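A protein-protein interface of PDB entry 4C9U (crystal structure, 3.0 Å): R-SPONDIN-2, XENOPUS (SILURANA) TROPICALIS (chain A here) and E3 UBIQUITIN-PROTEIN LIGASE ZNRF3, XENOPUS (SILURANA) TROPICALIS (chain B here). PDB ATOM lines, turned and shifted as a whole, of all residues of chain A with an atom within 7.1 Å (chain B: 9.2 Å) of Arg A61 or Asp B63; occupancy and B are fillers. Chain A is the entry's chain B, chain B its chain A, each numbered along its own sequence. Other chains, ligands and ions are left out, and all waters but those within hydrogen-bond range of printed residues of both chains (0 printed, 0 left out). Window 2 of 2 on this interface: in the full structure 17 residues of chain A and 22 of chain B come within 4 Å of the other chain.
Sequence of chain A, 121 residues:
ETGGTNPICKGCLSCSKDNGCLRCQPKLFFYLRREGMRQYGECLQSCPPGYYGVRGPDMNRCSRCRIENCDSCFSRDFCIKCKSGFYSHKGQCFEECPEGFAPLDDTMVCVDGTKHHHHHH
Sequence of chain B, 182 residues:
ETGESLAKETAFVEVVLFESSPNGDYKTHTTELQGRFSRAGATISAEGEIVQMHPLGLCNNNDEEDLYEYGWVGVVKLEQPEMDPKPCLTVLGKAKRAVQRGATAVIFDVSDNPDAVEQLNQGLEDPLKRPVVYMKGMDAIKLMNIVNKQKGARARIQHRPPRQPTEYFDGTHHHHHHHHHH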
ATOM      1  N   LEU A  28      15.373 -24.981  -7.970  1.00  0.00           N
ATOM      2  CA  LEU A  28      15.498 -26.211  -8.760  1.00  0.00           C
ATOM      3  C   LEU A  28      16.856 -26.309  -9.430  1.00  0.00           C
ATOM      4  O   LEU A  28      17.666 -25.385  -9.292  1.00  0.00           O
ATOM      5  CB  LEU A  28      14.369 -26.285  -9.814  1.00  0.00           C
ATOM      6  CG  LEU A  28      12.962 -26.044  -9.261  1.00  0.00           C
ATOM      7  CD1 LEU A  28      11.885 -26.275 -10.318  1.00  0.00           C
ATOM      8  CD2 LEU A  28      12.745 -26.931  -8.044  1.00  0.00           C
ATOM      9  N   PHE A  29      17.079 -27.415 -10.169  1.00  0.00           N
ATOM     10  CA  PHE A  29      18.370 -27.711 -10.835  1.00  0.00           C
ATOM     11  C   PHE A  29      18.322 -27.795 -12.401  1.00  0.00           C
ATOM     12  O   PHE A  29      17.503 -28.496 -12.987  1.00  0.00           O
ATOM     13  CB  PHE A  29      18.909 -29.022 -10.305  1.00  0.00           C
ATOM     14  CG  PHE A  29      19.441 -28.939  -8.921  1.00  0.00           C
ATOM     15  CD1 PHE A  29      18.587 -28.747  -7.856  1.00  0.00           C
ATOM     16  CD2 PHE A  29      20.786 -29.100  -8.659  1.00  0.00           C
ATOM     17  CE1 PHE A  29      19.062 -28.695  -6.559  1.00  0.00           C
ATOM     18  CE2 PHE A  29      21.267 -29.065  -7.355  1.00  0.00           C
ATOM     19  CZ  PHE A  29      20.402 -28.856  -6.310  1.00  0.00           C
ATOM     20  N   PHE A  30      19.269 -27.124 -13.045  1.00  0.00           N
ATOM     21  CA  PHE A  30      19.335 -27.054 -14.474  1.00  0.00           C
ATOM     22  C   PHE A  30      20.062 -28.292 -14.983  1.00  0.00           C
ATOM     23  O   PHE A  30      21.117 -28.643 -14.447  1.00  0.00           O
ATOM     24  CB  PHE A  30      20.071 -25.787 -14.918  1.00  0.00           C
ATOM     25  CG  PHE A  30      20.078 -25.570 -16.404  1.00  0.00           C
ATOM     26  CD1 PHE A  30      18.902 -25.253 -17.086  1.00  0.00           C
ATOM     27  CD2 PHE A  30      21.248 -25.669 -17.115  1.00  0.00           C
ATOM     28  CE1 PHE A  30      18.880 -25.053 -18.455  1.00  0.00           C
ATOM     29  CE2 PHE A  30      21.247 -25.464 -18.489  1.00  0.00           C
ATOM     30  CZ  PHE A  30      20.063 -25.155 -19.167  1.00  0.00           C
ATOM     31  N   TYR A  31      19.489 -28.928 -16.025  1.00  0.00           N
ATOM     32  CA  TYR A  31      19.981 -30.187 -16.556  1.00  0.00           C
ATOM     33  C   TYR A  31      19.875 -30.176 -18.043  1.00  0.00           C
ATOM     34  O   TYR A  31      18.767 -30.007 -18.584  1.00  0.00           O
ATOM     35  CB  TYR A  31      19.167 -31.346 -16.019  1.00  0.00           C
ATOM     36  CG  TYR A  31      19.401 -32.681 -16.721  1.00  0.00           C
ATOM     37  CD1 TYR A  31      20.647 -33.281 -16.711  1.00  0.00           C
ATOM     38  CD2 TYR A  31      18.350 -33.355 -17.374  1.00  0.00           C
ATOM     39  CE1 TYR A  31      20.856 -34.487 -17.332  1.00  0.00           C
ATOM     40  CE2 TYR A  31      18.542 -34.580 -17.988  1.00  0.00           C
ATOM     41  CZ  TYR A  31      19.806 -35.131 -17.978  1.00  0.00           C
ATOM     42  OH  TYR A  31      20.026 -36.333 -18.627  1.00  0.00           O
ATOM     43  N   LEU A  32      21.013 -30.409 -18.708  1.00  0.00           N
ATOM     44  CA  LEU A  32      21.053 -30.373 -20.147  1.00  0.00           C
ATOM     45  C   LEU A  32      20.874 -31.768 -20.733  1.00  0.00           C
ATOM     46  O   LEU A  32      21.795 -32.580 -20.759  1.00  0.00           O
ATOM     47  CB  LEU A  32      22.372 -29.805 -20.576  1.00  0.00           C
ATOM     48  CG  LEU A  32      22.546 -28.328 -20.265  1.00  0.00           C
ATOM     49  CD1 LEU A  32      23.984 -27.896 -20.456  1.00  0.00           C
ATOM     50  CD2 LEU A  32      21.625 -27.499 -21.139  1.00  0.00           C
ATOM     51  N   CYS A  47      18.636 -34.014  -8.959  1.00  0.00           N
ATOM     52  CA  CYS A  47      19.322 -34.418 -10.198  1.00  0.00           C
ATOM     53  C   CYS A  47      19.064 -35.872 -10.509  1.00  0.00           C
ATOM     54  O   CYS A  47      18.829 -36.666  -9.611  1.00  0.00           O
ATOM     55  CB  CYS A  47      20.828 -34.085 -10.168  1.00  0.00           C
ATOM     56  SG  CYS A  47      21.167 -32.295 -10.435  1.00  0.00           S
ATOM     57  N   TYR A  52      25.073 -35.497 -10.043  1.00  0.00           N
ATOM     58  CA  TYR A  52      25.017 -34.774  -8.808  1.00  0.00           C
ATOM     59  C   TYR A  52      24.814 -33.294  -9.102  1.00  0.00           C
ATOM     60  O   TYR A  52      25.100 -32.815 -10.201  1.00  0.00           O
ATOM     61  CB  TYR A  52      26.315 -34.979  -8.071  1.00  0.00           C
ATOM     62  CG  TYR A  52      27.494 -34.335  -8.742  1.00  0.00           C
ATOM     63  CD1 TYR A  52      27.852 -33.038  -8.443  1.00  0.00           C
ATOM     64  CD2 TYR A  52      28.245 -35.023  -9.663  1.00  0.00           C
ATOM     65  CE1 TYR A  52      28.933 -32.445  -9.052  1.00  0.00           C
ATOM     66  CE2 TYR A  52      29.324 -34.447 -10.280  1.00  0.00           C
ATOM     67  CZ  TYR A  52      29.669 -33.158  -9.956  1.00  0.00           C
ATOM     68  OH  TYR A  52      30.726 -32.546 -10.539  1.00  0.00           O
ATOM     69  N   GLY A  53      24.364 -32.569  -8.092  1.00  0.00           N
ATOM     70  CA  GLY A  53      24.112 -31.140  -8.240  1.00  0.00           C
ATOM     71  C   GLY A  53      25.126 -30.281  -7.533  1.00  0.00           C
ATOM     72  O   GLY A  53      25.810 -30.751  -6.622  1.00  0.00           O
ATOM     73  N   VAL A  54      25.230 -29.038  -8.010  1.00  0.00           N
ATOM     74  CA  VAL A  54      26.184 -28.047  -7.563  1.00  0.00           C
ATOM     75  C   VAL A  54      25.412 -26.737  -7.472  1.00  0.00           C
ATOM     76  O   VAL A  54      24.853 -26.266  -8.472  1.00  0.00           O
ATOM     77  CB  VAL A  54      27.318 -27.885  -8.589  1.00  0.00           C
ATOM     78  CG1 VAL A  54      28.176 -26.672  -8.271  1.00  0.00           C
ATOM     79  CG2 VAL A  54      28.177 -29.128  -8.628  1.00  0.00           C
ATOM     80  N   ARG A  55      25.370 -26.151  -6.276  1.00  0.00           N
ATOM     81  CA  ARG A  55      24.551 -24.961  -6.041  1.00  0.00           C
ATOM     82  C   ARG A  55      25.382 -23.729  -6.200  1.00  0.00           C
ATOM     83  O   ARG A  55      25.629 -23.026  -5.222  1.00  0.00           O
ATOM     84  CB  ARG A  55      23.913 -24.967  -4.639  1.00  0.00           C
ATOM     85  CG  ARG A  55      23.078 -26.195  -4.356  1.00  0.00           C
ATOM     86  CD  ARG A  55      22.212 -26.057  -3.089  1.00  0.00           C
ATOM     87  NE  ARG A  55      20.825 -26.117  -3.531  1.00  0.00           N
ATOM     88  CZ  ARG A  55      19.829 -26.794  -2.959  1.00  0.00           C
ATOM     89  NH1 ARG A  55      20.022 -27.504  -1.844  1.00  0.00           N
ATOM     90  NH2 ARG A  55      18.612 -26.761  -3.527  1.00  0.00           N
ATOM     91  N   GLY A  56      25.798 -23.454  -7.432  1.00  0.00           N
ATOM     92  CA  GLY A  56      26.597 -22.262  -7.717  1.00  0.00           C
ATOM     93  C   GLY A  56      25.953 -20.948  -7.246  1.00  0.00           C
ATOM     94  O   GLY A  56      24.744 -20.890  -6.937  1.00  0.00           O
ATOM     95  N   PRO A  57      26.768 -19.883  -7.148  1.00  0.00           N
ATOM     96  CA  PRO A  57      26.213 -18.616  -6.644  1.00  0.00           C
ATOM     97  C   PRO A  57      25.115 -18.113  -7.580  1.00  0.00           C
ATOM     98  O   PRO A  57      24.019 -17.739  -7.133  1.00  0.00           O
ATOM     99  CB  PRO A  57      27.429 -17.678  -6.626  1.00  0.00           C
ATOM    100  CG  PRO A  57      28.473 -18.328  -7.482  1.00  0.00           C
ATOM    101  CD  PRO A  57      28.204 -19.797  -7.492  1.00  0.00           C
ATOM    102  N   ASP A  58      25.429 -18.188  -8.876  1.00  0.00           N
ATOM    103  CA  ASP A  58      24.560 -17.747  -9.961  1.00  0.00           C
ATOM    104  C   ASP A  58      23.362 -18.700 -10.122  1.00  0.00           C
ATOM    105  O   ASP A  58      22.196 -18.284  -9.969  1.00  0.00           O
ATOM    106  CB  ASP A  58      25.386 -17.680 -11.267  1.00  0.00           C
ATOM    107  CG  ASP A  58      25.047 -16.480 -12.135  1.00  0.00           C
ATOM    108  OD1 ASP A  58      25.330 -15.344 -11.693  1.00  0.00           O
ATOM    109  OD2 ASP A  58      24.568 -16.664 -13.275  1.00  0.00           O
ATOM    110  N   MET A  59      23.660 -19.977 -10.397  1.00  0.00           N
ATOM    111  CA  MET A  59      22.627 -21.004 -10.666  1.00  0.00           C
ATOM    112  C   MET A  59      23.004 -22.421 -10.236  1.00  0.00           C
ATOM    113  O   MET A  59      24.167 -22.792 -10.226  1.00  0.00           O
ATOM    114  CB  MET A  59      22.328 -21.034 -12.160  1.00  0.00           C
ATOM    115  CG  MET A  59      23.349 -21.801 -12.986  1.00  0.00           C
ATOM    116  SD  MET A  59      23.107 -21.631 -14.753  1.00  0.00           S
ATOM    117  CE  MET A  59      21.449 -22.317 -14.933  1.00  0.00           C
ATOM    118  N   ASN A  60      21.998 -23.225  -9.953  1.00  0.00           N
ATOM    119  CA  ASN A  60      22.200 -24.620  -9.594  1.00  0.00           C
ATOM    120  C   ASN A  60      22.137 -25.483 -10.831  1.00  0.00           C
ATOM    121  O   ASN A  60      21.411 -25.178 -11.739  1.00  0.00           O
ATOM    122  CB  ASN A  60      21.125 -25.034  -8.618  1.00  0.00           C
ATOM    123  CG  ASN A  60      20.910 -24.001  -7.535  1.00  0.00           C
ATOM    124  OD1 ASN A  60      21.869 -23.514  -6.939  1.00  0.00           O
ATOM    125  ND2 ASN A  60      19.648 -23.633  -7.298  1.00  0.00           N
ATOM    126  N   ARG A  61      22.908 -26.555 -10.885  1.00  0.00           N
ATOM    127  CA  ARG A  61      22.930 -27.392 -12.093  1.00  0.00           C
ATOM    128  C   ARG A  61      23.490 -28.769 -11.859  1.00  0.00           C
ATOM    129  O   ARG A  61      24.206 -28.997 -10.896  1.00  0.00           O
ATOM    130  CB  ARG A  61      23.764 -26.729 -13.166  1.00  0.00           C
ATOM    131  CG  ARG A  61      25.228 -26.709 -12.818  1.00  0.00           C
ATOM    132  CD  ARG A  61      25.998 -26.040 -13.933  1.00  0.00           C
ATOM    133  NE  ARG A  61      27.394 -25.844 -13.543  1.00  0.00           N
ATOM    134  CZ  ARG A  61      27.827 -24.924 -12.675  1.00  0.00           C
ATOM    135  NH1 ARG A  61      26.978 -24.077 -12.074  1.00  0.00           N
ATOM    136  NH2 ARG A  61      29.129 -24.857 -12.398  1.00  0.00           N
ATOM    137  N   CYS A  62      23.175 -29.678 -12.765  1.00  0.00           N
ATOM    138  CA  CYS A  62      23.582 -31.068 -12.627  1.00  0.00           C
ATOM    139  C   CYS A  62      24.894 -31.295 -13.311  1.00  0.00           C
ATOM    140  O   CYS A  62      25.219 -30.615 -14.262  1.00  0.00           O
ATOM    141  CB  CYS A  62      22.529 -31.954 -13.245  1.00  0.00           C
ATOM    142  SG  CYS A  62      20.917 -31.789 -12.469  1.00  0.00           S
ATOM    143  N   SER A  63      25.683 -32.206 -12.786  1.00  0.00           N
ATOM    144  CA  SER A  63      26.844 -32.721 -13.507  1.00  0.00           C
ATOM    145  C   SER A  63      26.903 -34.231 -13.446  1.00  0.00           C
ATOM    146  O   SER A  63      26.512 -34.817 -12.464  1.00  0.00           O
ATOM    147  CB  SER A  63      28.140 -32.129 -12.912  1.00  0.00           C
ATOM    148  OG  SER A  63      28.818 -31.292 -13.837  1.00  0.00           O
ATOM    149  N   ARG A  66      31.147 -39.731 -13.300  1.00  0.00           N
ATOM    150  CA  ARG A  66      32.546 -39.982 -13.735  1.00  0.00           C
ATOM    151  C   ARG A  66      33.523 -40.580 -12.708  1.00  0.00           C
ATOM    152  O   ARG A  66      34.724 -40.402 -12.821  1.00  0.00           O
ATOM    153  CB  ARG A  66      33.194 -38.710 -14.287  1.00  0.00           C
ATOM    154  CG  ARG A  66      32.393 -37.989 -15.338  1.00  0.00           C
ATOM    155  CD  ARG A  66      33.221 -36.860 -15.943  1.00  0.00           C
ATOM    156  NE  ARG A  66      32.399 -35.987 -16.760  1.00  0.00           N
ATOM    157  CZ  ARG A  66      31.838 -36.338 -17.917  1.00  0.00           C
ATOM    158  NH1 ARG A  66      31.995 -37.562 -18.427  1.00  0.00           N
ATOM    159  NH2 ARG A  66      31.104 -35.447 -18.577  1.00  0.00           N
ATOM    160  N   ARG A  76      32.132 -33.861  -7.766  1.00  0.00           N
ATOM    161  CA  ARG A  76      32.858 -34.458  -8.908  1.00  0.00           C
ATOM    162  C   ARG A  76      33.891 -35.502  -8.507  1.00  0.00           C
ATOM    163  O   ARG A  76      34.128 -36.429  -9.267  1.00  0.00           O
ATOM    164  CB  ARG A  76      33.528 -33.373  -9.796  1.00  0.00           C
ATOM    165  CG  ARG A  76      34.967 -33.027  -9.484  1.00  0.00           C
ATOM    166  CD  ARG A  76      35.452 -31.839 -10.286  1.00  0.00           C
ATOM    167  NE  ARG A  76      35.914 -30.781  -9.371  1.00  0.00           N
ATOM    168  CZ  ARG A  76      35.537 -29.493  -9.394  1.00  0.00           C
ATOM    169  NH1 ARG A  76      34.706 -29.021 -10.330  1.00  0.00           N
ATOM    170  NH2 ARG A  76      36.031 -28.649  -8.479  1.00  0.00           N
ATOM    171  N   LEU B  56      23.555 -21.694 -22.692  1.00  0.00           N
ATOM    172  CA  LEU B  56      24.176 -21.887 -21.358  1.00  0.00           C
ATOM    173  C   LEU B  56      24.992 -23.166 -21.170  1.00  0.00           C
ATOM    174  O   LEU B  56      25.462 -23.441 -20.081  1.00  0.00           O
ATOM    175  CB  LEU B  56      23.114 -21.831 -20.269  1.00  0.00           C
ATOM    176  CG  LEU B  56      22.398 -20.488 -20.207  1.00  0.00           C
ATOM    177  CD1 LEU B  56      21.505 -20.481 -18.973  1.00  0.00           C
ATOM    178  CD2 LEU B  56      23.379 -19.311 -20.192  1.00  0.00           C
ATOM    179  N   GLY B  57      25.138 -23.960 -22.216  1.00  0.00           N
ATOM    180  CA  GLY B  57      26.027 -25.107 -22.172  1.00  0.00           C
ATOM    181  C   GLY B  57      27.457 -24.631 -22.264  1.00  0.00           C
ATOM    182  O   GLY B  57      28.383 -25.340 -21.898  1.00  0.00           O
ATOM    183  N   CYS B  59      29.824 -22.272 -20.931  1.00  0.00           N
ATOM    184  CA  CYS B  59      30.306 -21.340 -19.930  1.00  0.00           C
ATOM    185  C   CYS B  59      31.586 -21.881 -19.315  1.00  0.00           C
ATOM    186  O   CYS B  59      31.828 -23.089 -19.353  1.00  0.00           O
ATOM    187  CB  CYS B  59      29.237 -21.099 -18.864  1.00  0.00           C
ATOM    188  SG  CYS B  59      27.692 -20.325 -19.461  1.00  0.00           S
ATOM    189  N   ASN B  60      32.404 -20.978 -18.767  1.00  0.00           N
ATOM    190  CA  ASN B  60      33.692 -21.332 -18.137  1.00  0.00           C
ATOM    191  C   ASN B  60      33.607 -21.710 -16.670  1.00  0.00           C
ATOM    192  O   ASN B  60      34.389 -21.233 -15.849  1.00  0.00           O
ATOM    193  CB  ASN B  60      34.675 -20.194 -18.309  1.00  0.00           C
ATOM    194  CG  ASN B  60      35.246 -20.164 -19.692  1.00  0.00           C
ATOM    195  OD1 ASN B  60      35.470 -21.215 -20.294  1.00  0.00           O
ATOM    196  ND2 ASN B  60      35.466 -18.968 -20.221  1.00  0.00           N
ATOM    197  N   ASN B  61      32.683 -22.608 -16.365  1.00  0.00           N
ATOM    198  CA  ASN B  61      32.451 -23.080 -15.017  1.00  0.00           C
ATOM    199  C   ASN B  61      33.685 -23.749 -14.455  1.00  0.00           C
ATOM    200  O   ASN B  61      33.817 -23.876 -13.240  1.00  0.00           O
ATOM    201  CB  ASN B  61      31.337 -24.130 -14.986  1.00  0.00           C
ATOM    202  CG  ASN B  61      30.393 -24.035 -16.165  1.00  0.00           C
ATOM    203  OD1 ASN B  61      29.780 -22.995 -16.387  1.00  0.00           O
ATOM    204  ND2 ASN B  61      30.272 -25.126 -16.927  1.00  0.00           N
ATOM    205  N   ASN B  62      34.560 -24.212 -15.353  1.00  0.00           N
ATOM    206  CA  ASN B  62      35.610 -25.151 -15.014  1.00  0.00           C
ATOM    207  C   ASN B  62      35.045 -26.540 -14.674  1.00  0.00           C
ATOM    208  O   ASN B  62      35.814 -27.437 -14.361  1.00  0.00           O
ATOM    209  CB  ASN B  62      36.447 -24.602 -13.858  1.00  0.00           C
ATOM    210  CG  ASN B  62      37.847 -24.200 -14.280  1.00  0.00           C
ATOM    211  OD1 ASN B  62      38.563 -24.994 -14.904  1.00  0.00           O
ATOM    212  ND2 ASN B  62      38.260 -22.967 -13.919  1.00  0.00           N
ATOM    213  N   ASP B  63      33.719 -26.714 -14.743  1.00  0.00           N
ATOM    214  CA  ASP B  63      33.040 -27.934 -14.297  1.00  0.00           C
ATOM    215  C   ASP B  63      33.015 -29.015 -15.389  1.00  0.00           C
ATOM    216  O   ASP B  63      32.363 -28.835 -16.422  1.00  0.00           O
ATOM    217  CB  ASP B  63      31.611 -27.603 -13.827  1.00  0.00           C
ATOM    218  N   GLU B  64      33.703 -30.133 -15.130  1.00  0.00           N
ATOM    219  CA  GLU B  64      33.991 -31.167 -16.133  1.00  0.00           C
ATOM    220  C   GLU B  64      32.746 -31.509 -16.969  1.00  0.00           C
ATOM    221  O   GLU B  64      31.741 -31.948 -16.420  1.00  0.00           O
ATOM    222  CB  GLU B  64      34.562 -32.428 -15.449  1.00  0.00           C
ATOM    223  N   GLU B  65      32.814 -31.279 -18.284  1.00  0.00           N
ATOM    224  CA  GLU B  65      31.669 -31.504 -19.202  1.00  0.00           C
ATOM    225  C   GLU B  65      31.983 -32.719 -20.125  1.00  0.00           C
ATOM    226  O   GLU B  65      33.106 -33.241 -20.142  1.00  0.00           O
ATOM    227  CB  GLU B  65      31.269 -30.211 -19.990  1.00  0.00           C
ATOM    228  CG  GLU B  65      30.346 -29.247 -19.265  1.00  0.00           C
ATOM    229  N   ASP B  66      30.971 -33.202 -20.837  1.00  0.00           N
ATOM    230  CA  ASP B  66      31.124 -34.386 -21.656  1.00  0.00           C
ATOM    231  C   ASP B  66      32.152 -34.157 -22.752  1.00  0.00           C
ATOM    232  O   ASP B  66      32.287 -33.047 -23.290  1.00  0.00           O
ATOM    233  CB  ASP B  66      29.783 -34.816 -22.276  1.00  0.00           C
ATOM    234  CG  ASP B  66      28.866 -35.575 -21.290  1.00  0.00           C
ATOM    235  OD1 ASP B  66      29.351 -36.371 -20.474  1.00  0.00           O
ATOM    236  OD2 ASP B  66      27.635 -35.407 -21.345  1.00  0.00           O
ATOM    237  N   ARG B  97      34.742 -21.222 -26.753  1.00  0.00           N
ATOM    238  CA  ARG B  97      34.543 -22.406 -25.928  1.00  0.00           C
ATOM    239  C   ARG B  97      34.184 -23.631 -26.774  1.00  0.00           C
ATOM    240  O   ARG B  97      34.777 -24.689 -26.614  1.00  0.00           O
ATOM    241  CB  ARG B  97      33.429 -22.145 -24.902  1.00  0.00           C
ATOM    242  CG  ARG B  97      33.274 -23.212 -23.831  1.00  0.00           C
ATOM    243  CD  ARG B  97      34.258 -22.956 -22.711  1.00  0.00           C
ATOM    244  NE  ARG B  97      34.252 -24.032 -21.741  1.00  0.00           N
ATOM    245  CZ  ARG B  97      35.092 -25.054 -21.752  1.00  0.00           C
ATOM    246  NH1 ARG B  97      36.023 -25.170 -22.688  1.00  0.00           N
ATOM    247  NH2 ARG B  97      34.990 -25.977 -20.810  1.00  0.00           N
ATOM    248  N   ARG B 101      36.153 -27.322 -27.068  1.00  0.00           N
ATOM    249  CA  ARG B 101      35.534 -28.599 -26.831  1.00  0.00           C
ATOM    250  C   ARG B 101      35.391 -29.478 -28.095  1.00  0.00           C
ATOM    251  O   ARG B 101      34.727 -30.527 -28.077  1.00  0.00           O
ATOM    252  CB  ARG B 101      34.205 -28.380 -26.142  1.00  0.00           C
ATOM    253  CG  ARG B 101      34.380 -27.741 -24.766  1.00  0.00           C
ATOM    254  CD  ARG B 101      33.064 -27.532 -24.025  1.00  0.00           C
ATOM    255  NE  ARG B 101      32.326 -28.771 -23.926  1.00  0.00           N
ATOM    256  CZ  ARG B 101      31.049 -28.868 -23.561  1.00  0.00           C
ATOM    257  NH1 ARG B 101      30.339 -27.791 -23.219  1.00  0.00           N
ATOM    258  NH2 ARG B 101      30.476 -30.069 -23.527  1.00  0.00           N
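The guanidinium group (NH2) of Arg A66 sits close to the backbone carbonyl oxygen (O) of Glu B65, at 3.4 Å.
OD1 of Asp B66 is in salt-bridge range of NH2 of Arg A66 (2.7 Å).
The backbone carbonyl oxygen of Asp B66 sits at hydrogen-bond distance from the guanidinium group of Arg B101, 3.5 Å away.
O of Gly B57 lies within hydrogen-bond range of NH1 of Arg B101, 3.4 Å away.
N of Val A54 is in hydrogen-bond range of O of Arg A61, at 3.1 Å.
The backbone carbonyl oxygen (O) of Tyr A52 lies within hydrogen-bond range of the backbone NH (N) of Ser A63 (2.7 Å).
SG of Cys A47 forms a disulfide with SG of Cys A62 (2.1 Å).
Among the printed residues, merely in contact across the chains: Arg A61 with Asn B61, Leu A32 with Gly B57, Ser A63 with Glu B64 and Arg A61 with Asp B63.
Of the printed residues of chain A, Asp B63 touches Arg A61.
No residue of chain B comes within 4 Å of Gly A53.
No residue of chain B comes within 4 Å of Cys A62.
Printed residues of chain A within 4 Å of Asn B61: Arg A61 (3.5 Å).
Of the printed residues of chain B, Arg A66 touches Glu B65 and Asp B66.
Printed residues of chain A within 4 Å of Asp B66: Arg A66.
Printed residues of chain A within 4 Å of Glu B64: Ser A63.
Printed residues of chain B within 4 Å of Leu A32: Gly B57 (3.9 Å).
Arg B101 touches none of the printed residues of chain A.
Leu B56 touches none of the printed residues of chain A.
The nearest residue of chain B that does not touch Arg A61 is Asn B62 (6.2 Å).
Of the 12 printed residues of chain B, 6 touch a printed residue of chain A.
Printed residues of chain B that touch a printed residue of chain A: Gly B57, Asn B61, Asp B63, Glu B64, Glu B65 and Asp B66.
Among the printed residues, 6 pairs touch across the chains.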
